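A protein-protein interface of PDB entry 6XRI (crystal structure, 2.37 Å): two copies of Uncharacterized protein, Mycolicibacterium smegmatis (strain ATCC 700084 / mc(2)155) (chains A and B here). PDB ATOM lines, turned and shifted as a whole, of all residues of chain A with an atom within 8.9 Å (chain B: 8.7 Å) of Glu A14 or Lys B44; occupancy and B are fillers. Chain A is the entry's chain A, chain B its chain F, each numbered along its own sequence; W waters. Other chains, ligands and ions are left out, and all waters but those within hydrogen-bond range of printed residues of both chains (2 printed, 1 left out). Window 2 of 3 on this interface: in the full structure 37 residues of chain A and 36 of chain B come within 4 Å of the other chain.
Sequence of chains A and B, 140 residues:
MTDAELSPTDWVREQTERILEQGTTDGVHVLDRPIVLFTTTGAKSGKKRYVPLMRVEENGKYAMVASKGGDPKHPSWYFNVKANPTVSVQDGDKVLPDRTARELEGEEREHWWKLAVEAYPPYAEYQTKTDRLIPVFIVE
The backbone carbonyl oxygen (O) of Thr B41 lies within hydrogen-bond range of the side-chain amide nitrogen (ND2) of Asn B80. N of Lys B47 lies within hydrogen-bond range of OG of Ser B45, at 3.2 Å. NH1 of Arg B49 sits at hydrogen-bond distance from O of Lys B47, at 3.3 Å. The backbone carbonyl oxygen (O) of Lys B47 lies within hydrogen-bond range of the backbone NH (N) of Gly B42. The backbone carbonyl oxygen (O) of Arg A13 sits at hydrogen-bond distance from the side-chain hydroxyl (OG1) of Thr A16. The side-chain carboxylate of Glu A14 lies within salt-bridge range of the guanidinium group of Arg A18, at 2.6 Å.
No position is printed for both chains.
Water W1 lies within hydrogen-bond range of the side-chain carboxylate (OE2) of Glu A17 and the guanidinium group (NH2) of Arg B49. Water W2 bridges the backbone carbonyl oxygen of Ala B83 (3.3 Å) and the guanidinium group of Arg A13 (3.5 Å).
Lys B44 touches just these residues of chain A: Arg A13, Glu A14 and Glu A17. Of chain A, only Arg A13 and Glu A17 come within 4 Å of Ala B43. Ser B45 touches just one residue of chain A: Glu A17. Of the printed residues of chain B, Leu A20 touches Arg B49 (3.9 Å) and Asn B80 (3.6 Å). Printed residues of chain B within 4 Å of Glu A17: Gly B42, Ala B43, Lys B44, Ser B45, Arg B49 and Asn B80.
Hydrophobic or aromatic side chains of chain B within 4 Å of the printed part of chain A: Ala B43. Of the 16 printed residues of chain A, 5 touch a printed residue of chain B. Hydrophobic or aromatic side chains of chain A within 4 Å of the printed part of chain B: Leu A20. Along chain A the printed residues that touch a printed residue of chain B span positions 13 to 21. Among the printed residues, 12 pairs touch across the chains.
Arg A13 touches Ala B43 (O to CB, 3.5 Å). Arg A13 touches Lys B44. CD of Lys B44 touches CG of Glu A14 (3.8 Å). Glu A17 touches Gly B42 (OE1 to C, 3.3 Å). Glu A17 touches Asn B80 (CA to OD1, 3.8 Å). Leu A20 touches Arg B49 (CG to CG, 3.9 Å). Leu A20 touches Asn B80 (CD2 to OD1, 3.6 Å).
OE1 of Glu A17 sits at hydrogen-bond distance from N of Ala B43 (3.3 Å). OG of Ser B45 sits at hydrogen-bond distance from OE2 of Glu A17 (2.5 Å). OE1 of Glu A17 is in hydrogen-bond range of N of Lys B44 (2.7 Å). The side-chain carboxylate (OE2) of Glu A17 is in salt-bridge range of the guanidinium group (NH1) of Arg B49 (3.4 Å). OE1 of Glu A21 lies within salt-bridge range of NH2 of Arg B49 (2.7 Å).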
ATOM      1  N   LEU A   6     -30.680 -24.215  24.540  1.00  0.00           N
ATOM      2  CA  LEU A   6     -31.461 -23.224  23.788  1.00  0.00           C
ATOM      3  C   LEU A   6     -30.906 -21.798  24.009  1.00  0.00           C
ATOM      4  O   LEU A   6     -30.878 -20.981  23.068  1.00  0.00           O
ATOM      5  CB  LEU A   6     -32.955 -23.308  24.174  1.00  0.00           C
ATOM      6  CG  LEU A   6     -33.820 -24.018  23.124  1.00  0.00           C
ATOM      7  CD1 LEU A   6     -35.077 -24.612  23.724  1.00  0.00           C
ATOM      8  CD2 LEU A   6     -34.198 -23.053  22.003  1.00  0.00           C
ATOM      9  N   SER A   7     -30.495 -21.501  25.248  1.00  0.00           N
ATOM     10  CA  SER A   7     -29.768 -20.263  25.516  1.00  0.00           C
ATOM     11  C   SER A   7     -28.464 -20.309  24.729  1.00  0.00           C
ATOM     12  O   SER A   7     -27.807 -21.357  24.697  1.00  0.00           O
ATOM     13  CB  SER A   7     -29.500 -20.096  27.025  1.00  0.00           C
ATOM     14  OG  SER A   7     -28.409 -19.229  27.361  1.00  0.00           O
ATOM     15  N   PRO A   8     -28.059 -19.206  24.082  1.00  0.00           N
ATOM     16  CA  PRO A   8     -26.876 -19.280  23.193  1.00  0.00           C
ATOM     17  C   PRO A   8     -25.670 -19.897  23.889  1.00  0.00           C
ATOM     18  O   PRO A   8     -25.059 -20.824  23.345  1.00  0.00           O
ATOM     19  CB  PRO A   8     -26.647 -17.814  22.781  1.00  0.00           C
ATOM     20  CG  PRO A   8     -27.227 -17.008  23.938  1.00  0.00           C
ATOM     21  CD  PRO A   8     -28.427 -17.817  24.418  1.00  0.00           C
ATOM     22  N   THR A   9     -25.335 -19.404  25.094  1.00  0.00           N
ATOM     23  CA  THR A   9     -24.343 -20.014  25.972  1.00  0.00           C
ATOM     24  C   THR A   9     -24.439 -21.534  25.902  1.00  0.00           C
ATOM     25  O   THR A   9     -23.476 -22.218  25.542  1.00  0.00           O
ATOM     26  CB  THR A   9     -24.544 -19.511  27.411  1.00  0.00           C
ATOM     27  OG1 THR A   9     -24.506 -18.077  27.421  1.00  0.00           O
ATOM     28  CG2 THR A   9     -23.468 -20.081  28.319  1.00  0.00           C
ATOM     29  N   ASP A  10     -25.623 -22.069  26.186  1.00  0.00           N
ATOM     30  CA  ASP A  10     -25.787 -23.519  26.231  1.00  0.00           C
ATOM     31  C   ASP A  10     -25.785 -24.124  24.829  1.00  0.00           C
ATOM     32  O   ASP A  10     -25.501 -25.318  24.649  1.00  0.00           O
ATOM     33  CB  ASP A  10     -27.086 -23.840  26.977  1.00  0.00           C
ATOM     34  CG  ASP A  10     -27.040 -23.445  28.468  1.00  0.00           C
ATOM     35  OD1 ASP A  10     -25.942 -23.259  29.036  1.00  0.00           O
ATOM     36  OD2 ASP A  10     -28.127 -23.344  29.077  1.00  0.00           O
ATOM     37  N   TRP A  11     -26.134 -23.322  23.832  1.00  0.00           N
ATOM     38  CA  TRP A  11     -26.019 -23.793  22.464  1.00  0.00           C
ATOM     39  C   TRP A  11     -24.559 -24.011  22.124  1.00  0.00           C
ATOM     40  O   TRP A  11     -24.198 -25.011  21.499  1.00  0.00           O
ATOM     41  CB  TRP A  11     -26.660 -22.795  21.506  1.00  0.00           C
ATOM     42  CG  TRP A  11     -26.543 -23.206  20.082  1.00  0.00           C
ATOM     43  CD1 TRP A  11     -27.367 -24.050  19.406  1.00  0.00           C
ATOM     44  CD2 TRP A  11     -25.526 -22.802  19.161  1.00  0.00           C
ATOM     45  NE1 TRP A  11     -26.934 -24.191  18.115  1.00  0.00           N
ATOM     46  CE2 TRP A  11     -25.794 -23.445  17.947  1.00  0.00           C
ATOM     47  CE3 TRP A  11     -24.400 -21.966  19.251  1.00  0.00           C
ATOM     48  CZ2 TRP A  11     -25.002 -23.252  16.822  1.00  0.00           C
ATOM     49  CZ3 TRP A  11     -23.611 -21.784  18.129  1.00  0.00           C
ATOM     50  CH2 TRP A  11     -23.916 -22.420  16.938  1.00  0.00           C
ATOM     51  N   VAL A  12     -23.704 -23.104  22.576  1.00  0.00           N
ATOM     52  CA  VAL A  12     -22.275 -23.279  22.384  1.00  0.00           C
ATOM     53  C   VAL A  12     -21.778 -24.487  23.169  1.00  0.00           C
ATOM     54  O   VAL A  12     -21.161 -25.406  22.615  1.00  0.00           O
ATOM     55  CB  VAL A  12     -21.540 -21.986  22.770  1.00  0.00           C
ATOM     56  CG1 VAL A  12     -20.048 -22.263  23.042  1.00  0.00           C
ATOM     57  CG2 VAL A  12     -21.738 -20.961  21.642  1.00  0.00           C
ATOM     58  N   ARG A  13     -22.061 -24.516  24.466  1.00  0.00           N
ATOM     59  CA  ARG A  13     -21.610 -25.640  25.271  1.00  0.00           C
ATOM     60  C   ARG A  13     -22.069 -26.980  24.697  1.00  0.00           C
ATOM     61  O   ARG A  13     -21.345 -27.972  24.804  1.00  0.00           O
ATOM     62  CB  ARG A  13     -22.105 -25.500  26.698  1.00  0.00           C
ATOM     63  CG  ARG A  13     -21.709 -24.235  27.396  1.00  0.00           C
ATOM     64  CD  ARG A  13     -21.707 -24.498  28.882  1.00  0.00           C
ATOM     65  NE  ARG A  13     -21.602 -23.264  29.646  1.00  0.00           N
ATOM     66  CZ  ARG A  13     -21.404 -23.214  30.958  1.00  0.00           C
ATOM     67  NH1 ARG A  13     -21.284 -24.338  31.650  1.00  0.00           N
ATOM     68  NH2 ARG A  13     -21.316 -22.040  31.579  1.00  0.00           N
ATOM     69  N   GLU A  14     -23.264 -27.042  24.098  1.00  0.00           N
ATOM     70  CA  GLU A  14     -23.752 -28.305  23.540  1.00  0.00           C
ATOM     71  C   GLU A  14     -23.013 -28.683  22.260  1.00  0.00           C
ATOM     72  O   GLU A  14     -22.548 -29.820  22.104  1.00  0.00           O
ATOM     73  CB  GLU A  14     -25.254 -28.205  23.258  1.00  0.00           C
ATOM     74  CG  GLU A  14     -25.920 -29.508  22.884  1.00  0.00           C
ATOM     75  CD  GLU A  14     -27.427 -29.363  22.635  1.00  0.00           C
ATOM     76  OE1 GLU A  14     -28.144 -28.883  23.543  1.00  0.00           O
ATOM     77  OE2 GLU A  14     -27.902 -29.734  21.531  1.00  0.00           O
ATOM     78  N   GLN A  15     -22.951 -27.759  21.302  1.00  0.00           N
ATOM     79  CA  GLN A  15     -22.412 -28.106  19.991  1.00  0.00           C
ATOM     80  C   GLN A  15     -20.992 -28.635  20.117  1.00  0.00           C
ATOM     81  O   GLN A  15     -20.642 -29.656  19.510  1.00  0.00           O
ATOM     82  CB  GLN A  15     -22.460 -26.893  19.052  1.00  0.00           C
ATOM     83  CG  GLN A  15     -22.100 -27.188  17.576  1.00  0.00           C
ATOM     84  CD  GLN A  15     -23.035 -28.199  16.920  1.00  0.00           C
ATOM     85  OE1 GLN A  15     -23.850 -28.824  17.591  1.00  0.00           O
ATOM     86  NE2 GLN A  15     -22.925 -28.351  15.602  1.00  0.00           N
ATOM     87  N   THR A  16     -20.160 -27.957  20.905  1.00  0.00           N
ATOM     88  CA  THR A  16     -18.771 -28.374  21.009  1.00  0.00           C
ATOM     89  C   THR A  16     -18.685 -29.811  21.497  1.00  0.00           C
ATOM     90  O   THR A  16     -17.954 -30.633  20.927  1.00  0.00           O
ATOM     91  CB  THR A  16     -18.014 -27.446  21.949  1.00  0.00           C
ATOM     92  OG1 THR A  16     -18.547 -27.586  23.273  1.00  0.00           O
ATOM     93  CG2 THR A  16     -18.118 -25.995  21.496  1.00  0.00           C
ATOM     94  N   GLU A  17     -19.458 -30.138  22.536  1.00  0.00           N
ATOM     95  CA  GLU A  17     -19.529 -31.519  22.996  1.00  0.00           C
ATOM     96  C   GLU A  17     -19.983 -32.439  21.876  1.00  0.00           C
ATOM     97  O   GLU A  17     -19.466 -33.553  21.729  1.00  0.00           O
ATOM     98  CB  GLU A  17     -20.472 -31.635  24.188  1.00  0.00           C
ATOM     99  CG  GLU A  17     -20.702 -33.063  24.657  1.00  0.00           C
ATOM    100  CD  GLU A  17     -21.173 -33.102  26.105  1.00  0.00           C
ATOM    101  OE1 GLU A  17     -21.325 -32.016  26.694  1.00  0.00           O
ATOM    102  OE2 GLU A  17     -21.387 -34.197  26.662  1.00  0.00           O
ATOM    103  N   ARG A  18     -20.951 -31.988  21.073  1.00  0.00           N
ATOM    104  CA  ARG A  18     -21.418 -32.800  19.957  1.00  0.00           C
ATOM    105  C   ARG A  18     -20.274 -33.113  19.006  1.00  0.00           C
ATOM    106  O   ARG A  18     -20.178 -34.238  18.502  1.00  0.00           O
ATOM    107  CB  ARG A  18     -22.555 -32.086  19.230  1.00  0.00           C
ATOM    108  CG  ARG A  18     -23.116 -32.800  18.015  1.00  0.00           C
ATOM    109  CD  ARG A  18     -24.466 -32.166  17.662  1.00  0.00           C
ATOM    110  NE  ARG A  18     -25.466 -32.356  18.723  1.00  0.00           N
ATOM    111  CZ  ARG A  18     -26.457 -31.509  19.014  1.00  0.00           C
ATOM    112  NH1 ARG A  18     -26.609 -30.364  18.347  1.00  0.00           N
ATOM    113  NH2 ARG A  18     -27.293 -31.796  20.007  1.00  0.00           N
ATOM    114  N   ILE A  19     -19.384 -32.136  18.768  1.00  0.00           N
ATOM    115  CA  ILE A  19     -18.243 -32.352  17.875  1.00  0.00           C
ATOM    116  C   ILE A  19     -17.272 -33.347  18.502  1.00  0.00           C
ATOM    117  O   ILE A  19     -16.793 -34.277  17.844  1.00  0.00           O
ATOM    118  CB  ILE A  19     -17.546 -31.018  17.537  1.00  0.00           C
ATOM    119  CG1 ILE A  19     -18.514 -30.091  16.798  1.00  0.00           C
ATOM    120  CG2 ILE A  19     -16.296 -31.285  16.696  1.00  0.00           C
ATOM    121  CD1 ILE A  19     -17.921 -28.798  16.358  1.00  0.00           C
ATOM    122  N   LEU A  20     -16.977 -33.166  19.785  1.00  0.00           N
ATOM    123  CA  LEU A  20     -16.200 -34.143  20.532  1.00  0.00           C
ATOM    124  C   LEU A  20     -16.767 -35.552  20.347  1.00  0.00           C
ATOM    125  O   LEU A  20     -16.097 -36.450  19.822  1.00  0.00           O
ATOM    126  CB  LEU A  20     -16.194 -33.712  22.002  1.00  0.00           C
ATOM    127  CG  LEU A  20     -15.516 -34.572  23.056  1.00  0.00           C
ATOM    128  CD1 LEU A  20     -14.065 -34.737  22.769  1.00  0.00           C
ATOM    129  CD2 LEU A  20     -15.682 -33.943  24.454  1.00  0.00           C
ATOM    130  N   GLU A  21     -18.021 -35.750  20.744  1.00  0.00           N
ATOM    131  CA  GLU A  21     -18.621 -37.076  20.661  1.00  0.00           C
ATOM    132  C   GLU A  21     -18.534 -37.658  19.253  1.00  0.00           C
ATOM    133  O   GLU A  21     -18.485 -38.881  19.097  1.00  0.00           O
ATOM    134  CB  GLU A  21     -20.076 -37.013  21.129  1.00  0.00           C
ATOM    135  CG  GLU A  21     -20.880 -38.310  20.946  1.00  0.00           C
ATOM    136  CD  GLU A  21     -20.519 -39.389  21.951  1.00  0.00           C
ATOM    137  OE1 GLU A  21     -20.003 -39.022  23.046  1.00  0.00           O
ATOM    138  OE2 GLU A  21     -20.768 -40.581  21.623  1.00  0.00           O
ATOM    139  N   THR B  41     -13.676 -32.844  29.699  1.00  0.00           N
ATOM    140  CA  THR B  41     -15.027 -33.008  30.219  1.00  0.00           C
ATOM    141  C   THR B  41     -15.991 -32.292  29.286  1.00  0.00           C
ATOM    142  O   THR B  41     -15.869 -31.080  29.084  1.00  0.00           O
ATOM    143  CB  THR B  41     -15.135 -32.436  31.637  1.00  0.00           C
ATOM    144  OG1 THR B  41     -14.385 -33.246  32.548  1.00  0.00           O
ATOM    145  CG2 THR B  41     -16.569 -32.383  32.118  1.00  0.00           C
ATOM    146  N   GLY B  42     -16.948 -33.042  28.736  1.00  0.00           N
ATOM    147  CA  GLY B  42     -18.029 -32.502  27.928  1.00  0.00           C
ATOM    148  C   GLY B  42     -18.690 -31.278  28.523  1.00  0.00           C
ATOM    149  O   GLY B  42     -19.134 -31.303  29.673  1.00  0.00           O
ATOM    150  N   ALA B  43     -18.756 -30.191  27.756  1.00  0.00           N
ATOM    151  CA  ALA B  43     -19.173 -28.921  28.343  1.00  0.00           C
ATOM    152  C   ALA B  43     -20.637 -28.935  28.769  1.00  0.00           C
ATOM    153  O   ALA B  43     -21.005 -28.239  29.723  1.00  0.00           O
ATOM    154  CB  ALA B  43     -18.941 -27.775  27.366  1.00  0.00           C
ATOM    155  N   LYS B  44     -21.482 -29.703  28.083  1.00  0.00           N
ATOM    156  CA  LYS B  44     -22.912 -29.746  28.372  1.00  0.00           C
ATOM    157  C   LYS B  44     -23.326 -30.854  29.344  1.00  0.00           C
ATOM    158  O   LYS B  44     -24.171 -30.621  30.219  1.00  0.00           O
ATOM    159  CB  LYS B  44     -23.688 -29.911  27.064  1.00  0.00           C
ATOM    160  CG  LYS B  44     -25.118 -29.487  27.153  1.00  0.00           C
ATOM    161  CD  LYS B  44     -26.033 -30.526  26.580  1.00  0.00           C
ATOM    162  CE  LYS B  44     -27.375 -30.522  27.344  1.00  0.00           C
ATOM    163  NZ  LYS B  44     -28.279 -31.618  26.909  1.00  0.00           N
ATOM    164  N   SER B  45     -22.778 -32.063  29.194  1.00  0.00           N
ATOM    165  CA  SER B  45     -23.195 -33.206  29.992  1.00  0.00           C
ATOM    166  C   SER B  45     -22.247 -33.516  31.136  1.00  0.00           C
ATOM    167  O   SER B  45     -22.670 -34.130  32.113  1.00  0.00           O
ATOM    168  CB  SER B  45     -23.319 -34.457  29.119  1.00  0.00           C
ATOM    169  OG  SER B  45     -22.051 -35.039  28.897  1.00  0.00           O
ATOM    170  N   GLY B  46     -20.994 -33.092  31.056  1.00  0.00           N
ATOM    171  CA  GLY B  46     -20.043 -33.378  32.107  1.00  0.00           C
ATOM    172  C   GLY B  46     -19.313 -34.691  31.965  1.00  0.00           C
ATOM    173  O   GLY B  46     -18.506 -35.026  32.844  1.00  0.00           O
ATOM    174  N   LYS B  47     -19.597 -35.448  30.904  1.00  0.00           N
ATOM    175  CA  LYS B  47     -19.028 -36.769  30.691  1.00  0.00           C
ATOM    176  C   LYS B  47     -17.583 -36.635  30.238  1.00  0.00           C
ATOM    177  O   LYS B  47     -17.238 -35.731  29.472  1.00  0.00           O
ATOM    178  CB  LYS B  47     -19.867 -37.515  29.646  1.00  0.00           C
ATOM    179  CG  LYS B  47     -19.244 -38.765  29.047  1.00  0.00           C
ATOM    180  CD  LYS B  47     -20.220 -39.457  28.090  1.00  0.00           C
ATOM    181  CE  LYS B  47     -19.537 -40.549  27.256  1.00  0.00           C
ATOM    182  NZ  LYS B  47     -20.477 -41.280  26.339  1.00  0.00           N
ATOM    183  N   ARG B  49     -14.239 -37.512  28.311  1.00  0.00           N
ATOM    184  CA  ARG B  49     -13.612 -38.105  27.149  1.00  0.00           C
ATOM    185  C   ARG B  49     -12.116 -38.133  27.391  1.00  0.00           C
ATOM    186  O   ARG B  49     -11.583 -37.320  28.156  1.00  0.00           O
ATOM    187  CB  ARG B  49     -13.933 -37.322  25.881  1.00  0.00           C
ATOM    188  CG  ARG B  49     -15.262 -37.741  25.245  1.00  0.00           C
ATOM    189  CD  ARG B  49     -16.372 -37.892  26.277  1.00  0.00           C
ATOM    190  NE  ARG B  49     -17.672 -37.952  25.621  1.00  0.00           N
ATOM    191  CZ  ARG B  49     -18.602 -36.998  25.673  1.00  0.00           C
ATOM    192  NH1 ARG B  49     -18.411 -35.885  26.377  1.00  0.00           N
ATOM    193  NH2 ARG B  49     -19.747 -37.159  25.020  1.00  0.00           N
ATOM    194  N   ASN B  80     -14.072 -28.239  22.602  1.00  0.00           N
ATOM    195  CA  ASN B  80     -14.485 -28.559  23.963  1.00  0.00           C
ATOM    196  C   ASN B  80     -13.480 -28.060  24.993  1.00  0.00           C
ATOM    197  O   ASN B  80     -13.858 -27.445  25.996  1.00  0.00           O
ATOM    198  CB  ASN B  80     -14.673 -30.062  24.102  1.00  0.00           C
ATOM    199  CG  ASN B  80     -15.440 -30.421  25.336  1.00  0.00           C
ATOM    200  OD1 ASN B  80     -16.670 -30.553  25.300  1.00  0.00           O
ATOM    201  ND2 ASN B  80     -14.726 -30.564  26.453  1.00  0.00           N
ATOM    202  N   ALA B  83     -13.987 -24.447  25.533  1.00  0.00           N
ATOM    203  CA  ALA B  83     -15.156 -24.143  26.351  1.00  0.00           C
ATOM    204  C   ALA B  83     -14.912 -24.533  27.802  1.00  0.00           C
ATOM    205  O   ALA B  83     -15.236 -23.771  28.723  1.00  0.00           O
ATOM    206  CB  ALA B  83     -16.397 -24.861  25.812  1.00  0.00           C
ATOM    207  N   ASN B  84     -14.351 -25.725  28.031  1.00  0.00           N
ATOM    208  CA  ASN B  84     -14.100 -26.244  29.377  1.00  0.00           C
ATOM    209  C   ASN B  84     -12.601 -26.468  29.548  1.00  0.00           C
ATOM    210  O   ASN B  84     -12.065 -27.542  29.223  1.00  0.00           O
ATOM    211  CB  ASN B  84     -14.909 -27.516  29.638  1.00  0.00           C
ATOM    212  CG  ASN B  84     -14.877 -27.951  31.105  1.00  0.00           C
ATOM    213  OD1 ASN B  84     -14.297 -27.282  31.976  1.00  0.00           O
ATOM    214  ND2 ASN B  84     -15.511 -29.083  31.379  1.00  0.00           N
HETATM  215  O   HOH W   1     -22.339 -36.346  25.325  1.00  0.00           O
HETATM  216  O   HOH W   2     -18.076 -23.800  30.419  1.00  0.00           O
